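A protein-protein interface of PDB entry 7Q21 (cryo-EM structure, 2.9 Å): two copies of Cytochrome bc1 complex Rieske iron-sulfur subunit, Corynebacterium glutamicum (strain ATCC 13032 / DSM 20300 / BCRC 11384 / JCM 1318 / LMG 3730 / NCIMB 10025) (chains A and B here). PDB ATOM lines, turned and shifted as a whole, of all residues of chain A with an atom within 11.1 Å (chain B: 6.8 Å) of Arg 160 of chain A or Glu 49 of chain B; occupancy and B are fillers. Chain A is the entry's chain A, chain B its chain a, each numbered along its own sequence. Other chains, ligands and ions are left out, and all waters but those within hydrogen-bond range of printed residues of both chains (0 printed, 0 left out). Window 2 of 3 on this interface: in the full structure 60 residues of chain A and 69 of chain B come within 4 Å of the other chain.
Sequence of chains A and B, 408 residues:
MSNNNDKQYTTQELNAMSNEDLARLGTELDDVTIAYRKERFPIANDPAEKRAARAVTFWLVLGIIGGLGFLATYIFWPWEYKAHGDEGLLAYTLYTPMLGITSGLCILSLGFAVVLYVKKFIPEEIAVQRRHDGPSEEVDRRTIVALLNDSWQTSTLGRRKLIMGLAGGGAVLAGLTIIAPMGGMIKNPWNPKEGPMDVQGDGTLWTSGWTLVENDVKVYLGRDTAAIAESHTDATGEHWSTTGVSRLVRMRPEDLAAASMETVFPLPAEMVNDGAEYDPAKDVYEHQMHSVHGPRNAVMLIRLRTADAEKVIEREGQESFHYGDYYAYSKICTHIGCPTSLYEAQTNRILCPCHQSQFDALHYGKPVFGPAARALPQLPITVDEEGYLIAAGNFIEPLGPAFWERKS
The side-chain carboxylate (OE2) of Glu 49 of chain B lies within salt-bridge range of the guanidinium group (NH2) of Arg 160 of chain A (2.6 Å).
The backbone carbonyl oxygen (O) of Thr 156 of chain A lies within hydrogen-bond range of the side-chain hydroxyl (OH) of Tyr 117 of chain B, 2.7 Å away.
N of Leu 157 of chain A sits close to OH of Tyr 117 of chain B (3.5 Å).
The backbone carbonyl oxygen of Ser 155 of chain A lies within hydrogen-bond range of the side-chain hydroxyl of Tyr 117 of chain B.
The side-chain hydroxyl of Ser 155 of chain A lies close to the backbone NH of Leu 157 of chain A, 3.5 Å away.
The backbone carbonyl oxygen (O) of Thr 156 of chain A sits close to the guanidinium group (NE) of Arg 160 of chain A (3.1 Å).
OG of Ser 155 of chain A is in hydrogen-bond range of O of Trp 152 of chain A (2.9 Å).
Among the printed residues, pairs that only touch across the chains: Arg 160 of chain A with Phe 121 of chain B (3.1 Å), Ile 163 of chain A with Ala 53 of chain B (3.7 Å), Arg 160 of chain A with Phe 41 of chain B (3.8 Å) and Arg 160 of chain A with Tyr 117 of chain B (3.9 Å).
Printed residues of chain B within 4 Å of Ser 155 of chain A: Tyr 117 (3.2 Å).
Arg 160 of chain A touches just these residues of chain B: Phe 41 (3.8 Å), Glu 49 (2.6 Å), Tyr 117 (3.9 Å) and Phe 121 (3.1 Å).
Of the printed residues of chain A, Phe 41 of chain B touches Arg 160 (3.8 Å).
No residue of chain A comes within 4 Å of Asp 46 of chain B.
No residue of chain A comes within 4 Å of Pro 47 of chain B.
No residue of chain A comes within 4 Å of Ala 48 of chain B.
Glu 49 of chain B touches one residue of chain A.
No residue of chain A comes within 4 Å of Ala 52 of chain B.
The nearest residue of chain A that does not touch Glu 49 of chain B is Arg 159 of chain A (4.6 Å).
Printed residues of chain B that touch a printed residue of chain A: Phe 41, Glu 49, Ala 53, Tyr 117 and Phe 121.
Hydrophobic or aromatic side chains of chain B within 4 Å of the printed part of chain A: Phe 41, Tyr 117 and Phe 121.
Hydrophobic or aromatic side chains of chain A within 4 Å of the printed part of chain B: Leu 157 and Ile 163.
No position is printed for both chains.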
ATOM      1  N   TRP A 152     -11.045 -14.684   6.355  1.00  0.00           N
ATOM      2  CA  TRP A 152     -10.247 -13.501   6.063  1.00  0.00           C
ATOM      3  C   TRP A 152      -8.986 -13.451   6.925  1.00  0.00           C
ATOM      4  O   TRP A 152      -7.919 -13.113   6.422  1.00  0.00           O
ATOM      5  CB  TRP A 152     -11.081 -12.221   6.164  1.00  0.00           C
ATOM      6  CG  TRP A 152     -10.251 -10.982   6.022  1.00  0.00           C
ATOM      7  CD1 TRP A 152      -9.913 -10.106   7.011  1.00  0.00           C
ATOM      8  CD2 TRP A 152      -9.613 -10.499   4.825  1.00  0.00           C
ATOM      9  NE1 TRP A 152      -9.123  -9.105   6.515  1.00  0.00           N
ATOM     10  CE2 TRP A 152      -8.923  -9.317   5.176  1.00  0.00           C
ATOM     11  CE3 TRP A 152      -9.561 -10.940   3.495  1.00  0.00           C
ATOM     12  CZ2 TRP A 152      -8.198  -8.572   4.244  1.00  0.00           C
ATOM     13  CZ3 TRP A 152      -8.837 -10.209   2.576  1.00  0.00           C
ATOM     14  CH2 TRP A 152      -8.175  -9.034   2.946  1.00  0.00           C
ATOM     15  N   GLN A 153      -9.136 -13.762   8.221  1.00  0.00           N
ATOM     16  CA  GLN A 153      -8.051 -13.668   9.185  1.00  0.00           C
ATOM     17  C   GLN A 153      -6.978 -14.713   8.886  1.00  0.00           C
ATOM     18  O   GLN A 153      -5.790 -14.396   8.936  1.00  0.00           O
ATOM     19  CB  GLN A 153      -8.565 -13.809  10.624  1.00  0.00           C
ATOM     20  CG  GLN A 153      -9.376 -12.623  11.131  1.00  0.00           C
ATOM     21  CD  GLN A 153      -8.573 -11.349  11.217  1.00  0.00           C
ATOM     22  OE1 GLN A 153      -7.459 -11.318  11.738  1.00  0.00           O
ATOM     23  NE2 GLN A 153      -9.151 -10.270  10.720  1.00  0.00           N
ATOM     24  N   THR A 154      -7.402 -15.941   8.561  1.00  0.00           N
ATOM     25  CA  THR A 154      -6.480 -17.059   8.417  1.00  0.00           C
ATOM     26  C   THR A 154      -5.703 -16.957   7.105  1.00  0.00           C
ATOM     27  O   THR A 154      -4.605 -17.504   7.004  1.00  0.00           O
ATOM     28  CB  THR A 154      -7.180 -18.414   8.567  1.00  0.00           C
ATOM     29  OG1 THR A 154      -8.233 -18.472   7.610  1.00  0.00           O
ATOM     30  CG2 THR A 154      -7.743 -18.659   9.951  1.00  0.00           C
ATOM     31  N   SER A 155      -6.271 -16.244   6.119  1.00  0.00           N
ATOM     32  CA  SER A 155      -5.611 -16.020   4.838  1.00  0.00           C
ATOM     33  C   SER A 155      -4.347 -15.180   5.013  1.00  0.00           C
ATOM     34  O   SER A 155      -3.456 -15.231   4.169  1.00  0.00           O
ATOM     35  CB  SER A 155      -6.535 -15.385   3.834  1.00  0.00           C
ATOM     36  OG  SER A 155      -6.574 -13.977   4.007  1.00  0.00           O
ATOM     37  N   THR A 156      -4.297 -14.405   6.107  1.00  0.00           N
ATOM     38  CA  THR A 156      -3.186 -13.524   6.443  1.00  0.00           C
ATOM     39  C   THR A 156      -2.896 -12.601   5.261  1.00  0.00           C
ATOM     40  O   THR A 156      -1.777 -12.558   4.762  1.00  0.00           O
ATOM     41  CB  THR A 156      -1.947 -14.309   6.904  1.00  0.00           C
ATOM     42  OG1 THR A 156      -1.426 -15.032   5.788  1.00  0.00           O
ATOM     43  CG2 THR A 156      -2.234 -15.273   8.035  1.00  0.00           C
ATOM     44  N   LEU A 157      -3.929 -11.889   4.799  1.00  0.00           N
ATOM     45  CA  LEU A 157      -3.778 -10.954   3.693  1.00  0.00           C
ATOM     46  C   LEU A 157      -3.821  -9.509   4.188  1.00  0.00           C
ATOM     47  O   LEU A 157      -3.242  -8.631   3.553  1.00  0.00           O
ATOM     48  CB  LEU A 157      -4.836 -11.237   2.619  1.00  0.00           C
ATOM     49  CG  LEU A 157      -4.737 -10.419   1.326  1.00  0.00           C
ATOM     50  CD1 LEU A 157      -3.329 -10.407   0.747  1.00  0.00           C
ATOM     51  CD2 LEU A 157      -5.724 -10.926   0.286  1.00  0.00           C
ATOM     52  N   GLY A 158      -4.494  -9.283   5.323  1.00  0.00           N
ATOM     53  CA  GLY A 158      -4.606  -7.980   5.963  1.00  0.00           C
ATOM     54  C   GLY A 158      -3.259  -7.388   6.374  1.00  0.00           C
ATOM     55  O   GLY A 158      -3.121  -6.163   6.431  1.00  0.00           O
ATOM     56  N   ARG A 159      -2.283  -8.267   6.641  1.00  0.00           N
ATOM     57  CA  ARG A 159      -0.985  -7.838   7.149  1.00  0.00           C
ATOM     58  C   ARG A 159      -0.062  -7.463   5.991  1.00  0.00           C
ATOM     59  O   ARG A 159       0.876  -6.690   6.179  1.00  0.00           O
ATOM     60  CB  ARG A 159      -0.337  -8.898   8.041  1.00  0.00           C
ATOM     61  CG  ARG A 159      -1.290  -9.544   9.037  1.00  0.00           C
ATOM     62  CD  ARG A 159      -0.614 -10.303  10.169  1.00  0.00           C
ATOM     63  NE  ARG A 159       0.141 -11.502   9.805  1.00  0.00           N
ATOM     64  CZ  ARG A 159      -0.317 -12.751   9.851  1.00  0.00           C
ATOM     65  NH1 ARG A 159       0.473 -13.748   9.491  1.00  0.00           N
ATOM     66  NH2 ARG A 159      -1.551 -13.006  10.253  1.00  0.00           N
ATOM     67  N   ARG A 160      -0.344  -8.011   4.805  1.00  0.00           N
ATOM     68  CA  ARG A 160       0.502  -7.785   3.648  1.00  0.00           C
ATOM     69  C   ARG A 160      -0.050  -6.586   2.894  1.00  0.00           C
ATOM     70  O   ARG A 160      -0.952  -6.722   2.074  1.00  0.00           O
ATOM     71  CB  ARG A 160       0.565  -9.044   2.783  1.00  0.00           C
ATOM     72  CG  ARG A 160       1.471 -10.147   3.305  1.00  0.00           C
ATOM     73  CD  ARG A 160       0.610 -11.119   4.074  1.00  0.00           C
ATOM     74  NE  ARG A 160       1.282 -12.360   4.428  1.00  0.00           N
ATOM     75  CZ  ARG A 160       2.098 -12.523   5.466  1.00  0.00           C
ATOM     76  NH1 ARG A 160       2.355 -11.526   6.297  1.00  0.00           N
ATOM     77  NH2 ARG A 160       2.642 -13.706   5.688  1.00  0.00           N
ATOM     78  N   LYS A 161       0.466  -5.402   3.222  1.00  0.00           N
ATOM     79  CA  LYS A 161       0.013  -4.163   2.603  1.00  0.00           C
ATOM     80  C   LYS A 161       0.467  -4.095   1.144  1.00  0.00           C
ATOM     81  O   LYS A 161      -0.297  -3.690   0.267  1.00  0.00           O
ATOM     82  CB  LYS A 161       0.503  -2.945   3.394  1.00  0.00           C
ATOM     83  CG  LYS A 161      -0.118  -2.717   4.768  1.00  0.00           C
ATOM     84  CD  LYS A 161      -1.634  -2.702   4.794  1.00  0.00           C
ATOM     85  CE  LYS A 161      -2.193  -2.352   6.156  1.00  0.00           C
ATOM     86  NZ  LYS A 161      -3.675  -2.403   6.167  1.00  0.00           N
ATOM     87  N   LEU A 162       1.705  -4.541   0.899  1.00  0.00           N
ATOM     88  CA  LEU A 162       2.297  -4.455  -0.424  1.00  0.00           C
ATOM     89  C   LEU A 162       1.610  -5.422  -1.380  1.00  0.00           C
ATOM     90  O   LEU A 162       1.343  -5.051  -2.521  1.00  0.00           O
ATOM     91  CB  LEU A 162       3.809  -4.706  -0.365  1.00  0.00           C
ATOM     92  CG  LEU A 162       4.542  -4.473  -1.688  1.00  0.00           C
ATOM     93  CD1 LEU A 162       4.329  -3.051  -2.189  1.00  0.00           C
ATOM     94  CD2 LEU A 162       6.029  -4.763  -1.546  1.00  0.00           C
ATOM     95  N   ILE A 163       1.319  -6.638  -0.898  1.00  0.00           N
ATOM     96  CA  ILE A 163       0.786  -7.701  -1.740  1.00  0.00           C
ATOM     97  C   ILE A 163      -0.607  -7.296  -2.218  1.00  0.00           C
ATOM     98  O   ILE A 163      -0.906  -7.382  -3.407  1.00  0.00           O
ATOM     99  CB  ILE A 163       0.785  -9.076  -1.027  1.00  0.00           C
ATOM    100  CG1 ILE A 163       2.152  -9.513  -0.482  1.00  0.00           C
ATOM    101  CG2 ILE A 163       0.138 -10.148  -1.894  1.00  0.00           C
ATOM    102  CD1 ILE A 163       3.330  -9.299  -1.409  1.00  0.00           C
ATOM    103  N   MET A 164      -1.440  -6.827  -1.285  1.00  0.00           N
ATOM    104  CA  MET A 164      -2.813  -6.471  -1.599  1.00  0.00           C
ATOM    105  C   MET A 164      -2.848  -5.157  -2.375  1.00  0.00           C
ATOM    106  O   MET A 164      -3.731  -4.979  -3.209  1.00  0.00           O
ATOM    107  CB  MET A 164      -3.722  -6.435  -0.363  1.00  0.00           C
ATOM    108  CG  MET A 164      -3.623  -5.177   0.473  1.00  0.00           C
ATOM    109  SD  MET A 164      -5.107  -4.930   1.479  1.00  0.00           S
ATOM    110  CE  MET A 164      -4.645  -5.833   2.953  1.00  0.00           C
ATOM    111  N   GLY A 165      -1.889  -4.254  -2.113  1.00  0.00           N
ATOM    112  CA  GLY A 165      -1.766  -3.014  -2.867  1.00  0.00           C
ATOM    113  C   GLY A 165      -1.441  -3.273  -4.338  1.00  0.00           C
ATOM    114  O   GLY A 165      -2.062  -2.698  -5.228  1.00  0.00           O
ATOM    115  N   LEU A 166      -0.462  -4.155  -4.570  1.00  0.00           N
ATOM    116  CA  LEU A 166      -0.034  -4.497  -5.918  1.00  0.00           C
ATOM    117  C   LEU A 166      -1.101  -5.341  -6.611  1.00  0.00           C
ATOM    118  O   LEU A 166      -1.254  -5.245  -7.824  1.00  0.00           O
ATOM    119  CB  LEU A 166       1.319  -5.216  -5.884  1.00  0.00           C
ATOM    120  CG  LEU A 166       2.544  -4.363  -5.554  1.00  0.00           C
ATOM    121  CD1 LEU A 166       3.810  -5.198  -5.656  1.00  0.00           C
ATOM    122  CD2 LEU A 166       2.637  -3.146  -6.461  1.00  0.00           C
ATOM    123  N   ALA A 167      -1.824  -6.163  -5.837  1.00  0.00           N
ATOM    124  CA  ALA A 167      -2.878  -7.012  -6.372  1.00  0.00           C
ATOM    125  C   ALA A 167      -4.022  -6.160  -6.914  1.00  0.00           C
ATOM    126  O   ALA A 167      -4.561  -6.479  -7.970  1.00  0.00           O
ATOM    127  CB  ALA A 167      -3.360  -8.000  -5.333  1.00  0.00           C
ATOM    128  N   GLY A 168      -4.373  -5.088  -6.187  1.00  0.00           N
ATOM    129  CA  GLY A 168      -5.394  -4.146  -6.619  1.00  0.00           C
ATOM    130  C   GLY A 168      -5.037  -3.502  -7.959  1.00  0.00           C
ATOM    131  O   GLY A 168      -5.850  -3.465  -8.882  1.00  0.00           O
ATOM    132  N   PHE B  41       2.989 -21.232   8.519  1.00  0.00           N
ATOM    133  CA  PHE B  41       4.235 -21.217   9.269  1.00  0.00           C
ATOM    134  C   PHE B  41       4.002 -20.499  10.597  1.00  0.00           C
ATOM    135  O   PHE B  41       3.717 -19.302  10.624  1.00  0.00           O
ATOM    136  CB  PHE B  41       5.372 -20.651   8.409  1.00  0.00           C
ATOM    137  CG  PHE B  41       5.097 -19.252   7.931  1.00  0.00           C
ATOM    138  CD1 PHE B  41       4.377 -19.016   6.766  1.00  0.00           C
ATOM    139  CD2 PHE B  41       5.501 -18.172   8.699  1.00  0.00           C
ATOM    140  CE1 PHE B  41       4.102 -17.718   6.363  1.00  0.00           C
ATOM    141  CE2 PHE B  41       5.205 -16.876   8.310  1.00  0.00           C
ATOM    142  CZ  PHE B  41       4.499 -16.654   7.144  1.00  0.00           C
ATOM    143  N   ILE B  43       6.175 -19.585  12.784  1.00  0.00           N
ATOM    144  CA  ILE B  43       7.489 -19.128  13.201  1.00  0.00           C
ATOM    145  C   ILE B  43       7.486 -17.604  13.209  1.00  0.00           C
ATOM    146  O   ILE B  43       7.036 -16.972  12.251  1.00  0.00           O
ATOM    147  CB  ILE B  43       8.597 -19.703  12.290  1.00  0.00           C
ATOM    148  CG1 ILE B  43       8.494 -21.225  12.124  1.00  0.00           C
ATOM    149  CG2 ILE B  43       9.989 -19.260  12.736  1.00  0.00           C
ATOM    150  CD1 ILE B  43       8.833 -22.045  13.360  1.00  0.00           C
ATOM    151  N   ALA B  44       8.018 -17.035  14.299  1.00  0.00           N
ATOM    152  CA  ALA B  44       8.257 -15.603  14.405  1.00  0.00           C
ATOM    153  C   ALA B  44       9.321 -15.190  13.394  1.00  0.00           C
ATOM    154  O   ALA B  44      10.441 -15.694  13.426  1.00  0.00           O
ATOM    155  CB  ALA B  44       8.639 -15.235  15.816  1.00  0.00           C
ATOM    156  N   ASN B  45       8.901 -14.336  12.453  1.00  0.00           N
ATOM    157  CA  ASN B  45       9.697 -13.664  11.439  1.00  0.00           C
ATOM    158  C   ASN B  45      10.801 -14.544  10.858  1.00  0.00           C
ATOM    159  O   ASN B  45      11.980 -14.192  10.920  1.00  0.00           O
ATOM    160  CB  ASN B  45      10.174 -12.290  11.911  1.00  0.00           C
ATOM    161  CG  ASN B  45      11.106 -12.306  13.105  1.00  0.00           C
ATOM    162  OD1 ASN B  45      11.392 -13.346  13.691  1.00  0.00           O
ATOM    163  ND2 ASN B  45      11.618 -11.140  13.458  1.00  0.00           N
ATOM    164  N   ASP B  46      10.394 -15.692  10.302  1.00  0.00           N
ATOM    165  CA  ASP B  46      11.312 -16.556   9.585  1.00  0.00           C
ATOM    166  C   ASP B  46      11.540 -15.977   8.190  1.00  0.00           C
ATOM    167  O   ASP B  46      10.656 -15.336   7.632  1.00  0.00           O
ATOM    168  CB  ASP B  46      10.770 -17.987   9.517  1.00  0.00           C
ATOM    169  CG  ASP B  46       9.384 -18.087   8.916  1.00  0.00           C
ATOM    170  OD1 ASP B  46       8.618 -17.120   9.052  1.00  0.00           O
ATOM    171  OD2 ASP B  46       9.113 -19.094   8.253  1.00  0.00           O
ATOM    172  N   PRO B  47      12.747 -16.146   7.606  1.00  0.00           N
ATOM    173  CA  PRO B  47      13.026 -15.692   6.242  1.00  0.00           C
ATOM    174  C   PRO B  47      12.155 -16.306   5.149  1.00  0.00           C
ATOM    175  O   PRO B  47      12.059 -15.731   4.068  1.00  0.00           O
ATOM    176  CB  PRO B  47      14.497 -16.083   6.029  1.00  0.00           C
ATOM    177  CG  PRO B  47      15.064 -16.126   7.424  1.00  0.00           C
ATOM    178  CD  PRO B  47      13.940 -16.727   8.235  1.00  0.00           C
ATOM    179  N   ALA B  48      11.489 -17.433   5.450  1.00  0.00           N
ATOM    180  CA  ALA B  48      10.665 -18.136   4.470  1.00  0.00           C
ATOM    181  C   ALA B  48       9.389 -17.365   4.128  1.00  0.00           C
ATOM    182  O   ALA B  48       8.908 -17.434   2.998  1.00  0.00           O
ATOM    183  CB  ALA B  48      10.370 -19.541   4.917  1.00  0.00           C
ATOM    184  N   GLU B  49       8.875 -16.606   5.108  1.00  0.00           N
ATOM    185  CA  GLU B  49       7.761 -15.695   4.897  1.00  0.00           C
ATOM    186  C   GLU B  49       8.162 -14.636   3.878  1.00  0.00           C
ATOM    187  O   GLU B  49       7.378 -14.352   2.979  1.00  0.00           O
ATOM    188  CB  GLU B  49       7.339 -15.057   6.222  1.00  0.00           C
ATOM    189  CG  GLU B  49       6.284 -13.961   6.100  1.00  0.00           C
ATOM    190  CD  GLU B  49       5.617 -13.579   7.410  1.00  0.00           C
ATOM    191  OE1 GLU B  49       6.232 -13.786   8.471  1.00  0.00           O
ATOM    192  OE2 GLU B  49       4.467 -13.098   7.373  1.00  0.00           O
ATOM    193  N   LYS B  50       9.364 -14.065   4.037  1.00  0.00           N
ATOM    194  CA  LYS B  50       9.834 -13.008   3.158  1.00  0.00           C
ATOM    195  C   LYS B  50      10.048 -13.571   1.755  1.00  0.00           C
ATOM    196  O   LYS B  50       9.699 -12.924   0.767  1.00  0.00           O
ATOM    197  CB  LYS B  50      11.099 -12.351   3.719  1.00  0.00           C
ATOM    198  CG  LYS B  50      11.162 -12.158   5.230  1.00  0.00           C
ATOM    199  CD  LYS B  50      10.139 -11.183   5.776  1.00  0.00           C
ATOM    200  CE  LYS B  50      10.057 -11.201   7.288  1.00  0.00           C
ATOM    201  NZ  LYS B  50       8.897 -10.424   7.785  1.00  0.00           N
ATOM    202  N   ARG B  51      10.463 -14.850   1.691  1.00  0.00           N
ATOM    203  CA  ARG B  51      10.737 -15.518   0.427  1.00  0.00           C
ATOM    204  C   ARG B  51       9.441 -15.749  -0.347  1.00  0.00           C
ATOM    205  O   ARG B  51       9.378 -15.467  -1.547  1.00  0.00           O
ATOM    206  CB  ARG B  51      11.480 -16.832   0.675  1.00  0.00           C
ATOM    207  CG  ARG B  51      12.978 -16.665   0.885  1.00  0.00           C
ATOM    208  CD  ARG B  51      13.786 -17.924   0.594  1.00  0.00           C
ATOM    209  NE  ARG B  51      13.482 -19.034   1.493  1.00  0.00           N
ATOM    210  CZ  ARG B  51      13.955 -19.177   2.725  1.00  0.00           C
ATOM    211  NH1 ARG B  51      14.798 -18.297   3.242  1.00  0.00           N
ATOM    212  NH2 ARG B  51      13.587 -20.217   3.452  1.00  0.00           N
ATOM    213  N   ALA B  52       8.408 -16.211   0.370  1.00  0.00           N
ATOM    214  CA  ALA B  52       7.096 -16.437  -0.215  1.00  0.00           C
ATOM    215  C   ALA B  52       6.480 -15.112  -0.663  1.00  0.00           C
ATOM    216  O   ALA B  52       5.782 -15.063  -1.669  1.00  0.00           O
ATOM    217  CB  ALA B  52       6.208 -17.177   0.755  1.00  0.00           C
ATOM    218  N   ALA B  53       6.713 -14.053   0.118  1.00  0.00           N
ATOM    219  CA  ALA B  53       6.173 -12.737  -0.181  1.00  0.00           C
ATOM    220  C   ALA B  53       6.881 -12.144  -1.393  1.00  0.00           C
ATOM    221  O   ALA B  53       6.252 -11.438  -2.171  1.00  0.00           O
ATOM    222  CB  ALA B  53       6.235 -11.839   1.029  1.00  0.00           C
ATOM    223  N   ARG B  54       8.175 -12.451  -1.550  1.00  0.00           N
ATOM    224  CA  ARG B  54       8.978 -11.904  -2.631  1.00  0.00           C
ATOM    225  C   ARG B  54       8.767 -12.666  -3.937  1.00  0.00           C
ATOM    226  O   ARG B  54       9.347 -12.263  -4.940  1.00  0.00           O
ATOM    227  CB  ARG B  54      10.466 -11.858  -2.257  1.00  0.00           C
ATOM    228  CG  ARG B  54      10.842 -10.673  -1.379  1.00  0.00           C
ATOM    229  CD  ARG B  54      12.317 -10.354  -1.359  1.00  0.00           C
ATOM    230  NE  ARG B  54      12.967 -10.931  -0.188  1.00  0.00           N
ATOM    231  CZ  ARG B  54      13.692 -12.047  -0.175  1.00  0.00           C
ATOM    232  NH1 ARG B  54      13.851 -12.754  -1.282  1.00  0.00           N
ATOM    233  NH2 ARG B  54      14.235 -12.466   0.954  1.00  0.00           N
ATOM    234  N   TYR B 117      -0.123 -17.532  -4.040  1.00  0.00           N
ATOM    235  CA  TYR B 117      -0.558 -17.026  -2.745  1.00  0.00           C
ATOM    236  C   TYR B 117      -1.348 -18.091  -1.992  1.00  0.00           C
ATOM    237  O   TYR B 117      -1.183 -18.239  -0.784  1.00  0.00           O
ATOM    238  CB  TYR B 117      -1.353 -15.720  -2.865  1.00  0.00           C
ATOM    239  CG  TYR B 117      -1.565 -15.027  -1.541  1.00  0.00           C
ATOM    240  CD1 TYR B 117      -2.658 -15.322  -0.737  1.00  0.00           C
ATOM    241  CD2 TYR B 117      -0.649 -14.096  -1.073  1.00  0.00           C
ATOM    242  CE1 TYR B 117      -2.835 -14.714   0.497  1.00  0.00           C
ATOM    243  CE2 TYR B 117      -0.814 -13.475   0.156  1.00  0.00           C
ATOM    244  CZ  TYR B 117      -1.909 -13.788   0.943  1.00  0.00           C
ATOM    245  OH  TYR B 117      -2.078 -13.186   2.153  1.00  0.00           O
ATOM    246  N   PHE B 121       0.388 -19.205   1.465  1.00  0.00           N
ATOM    247  CA  PHE B 121      -0.064 -18.376   2.578  1.00  0.00           C
ATOM    248  C   PHE B 121      -1.352 -18.881   3.222  1.00  0.00           C
ATOM    249  O   PHE B 121      -1.497 -18.807   4.441  1.00  0.00           O
ATOM    250  CB  PHE B 121      -0.196 -16.910   2.160  1.00  0.00           C
ATOM    251  CG  PHE B 121       1.116 -16.182   2.047  1.00  0.00           C
ATOM    252  CD1 PHE B 121       1.608 -15.801   0.808  1.00  0.00           C
ATOM    253  CD2 PHE B 121       1.868 -15.890   3.179  1.00  0.00           C
ATOM    254  CE1 PHE B 121       2.815 -15.127   0.704  1.00  0.00           C
ATOM    255  CE2 PHE B 121       3.079 -15.223   3.071  1.00  0.00           C
ATOM    256  CZ  PHE B 121       3.547 -14.838   1.836  1.00  0.00           C
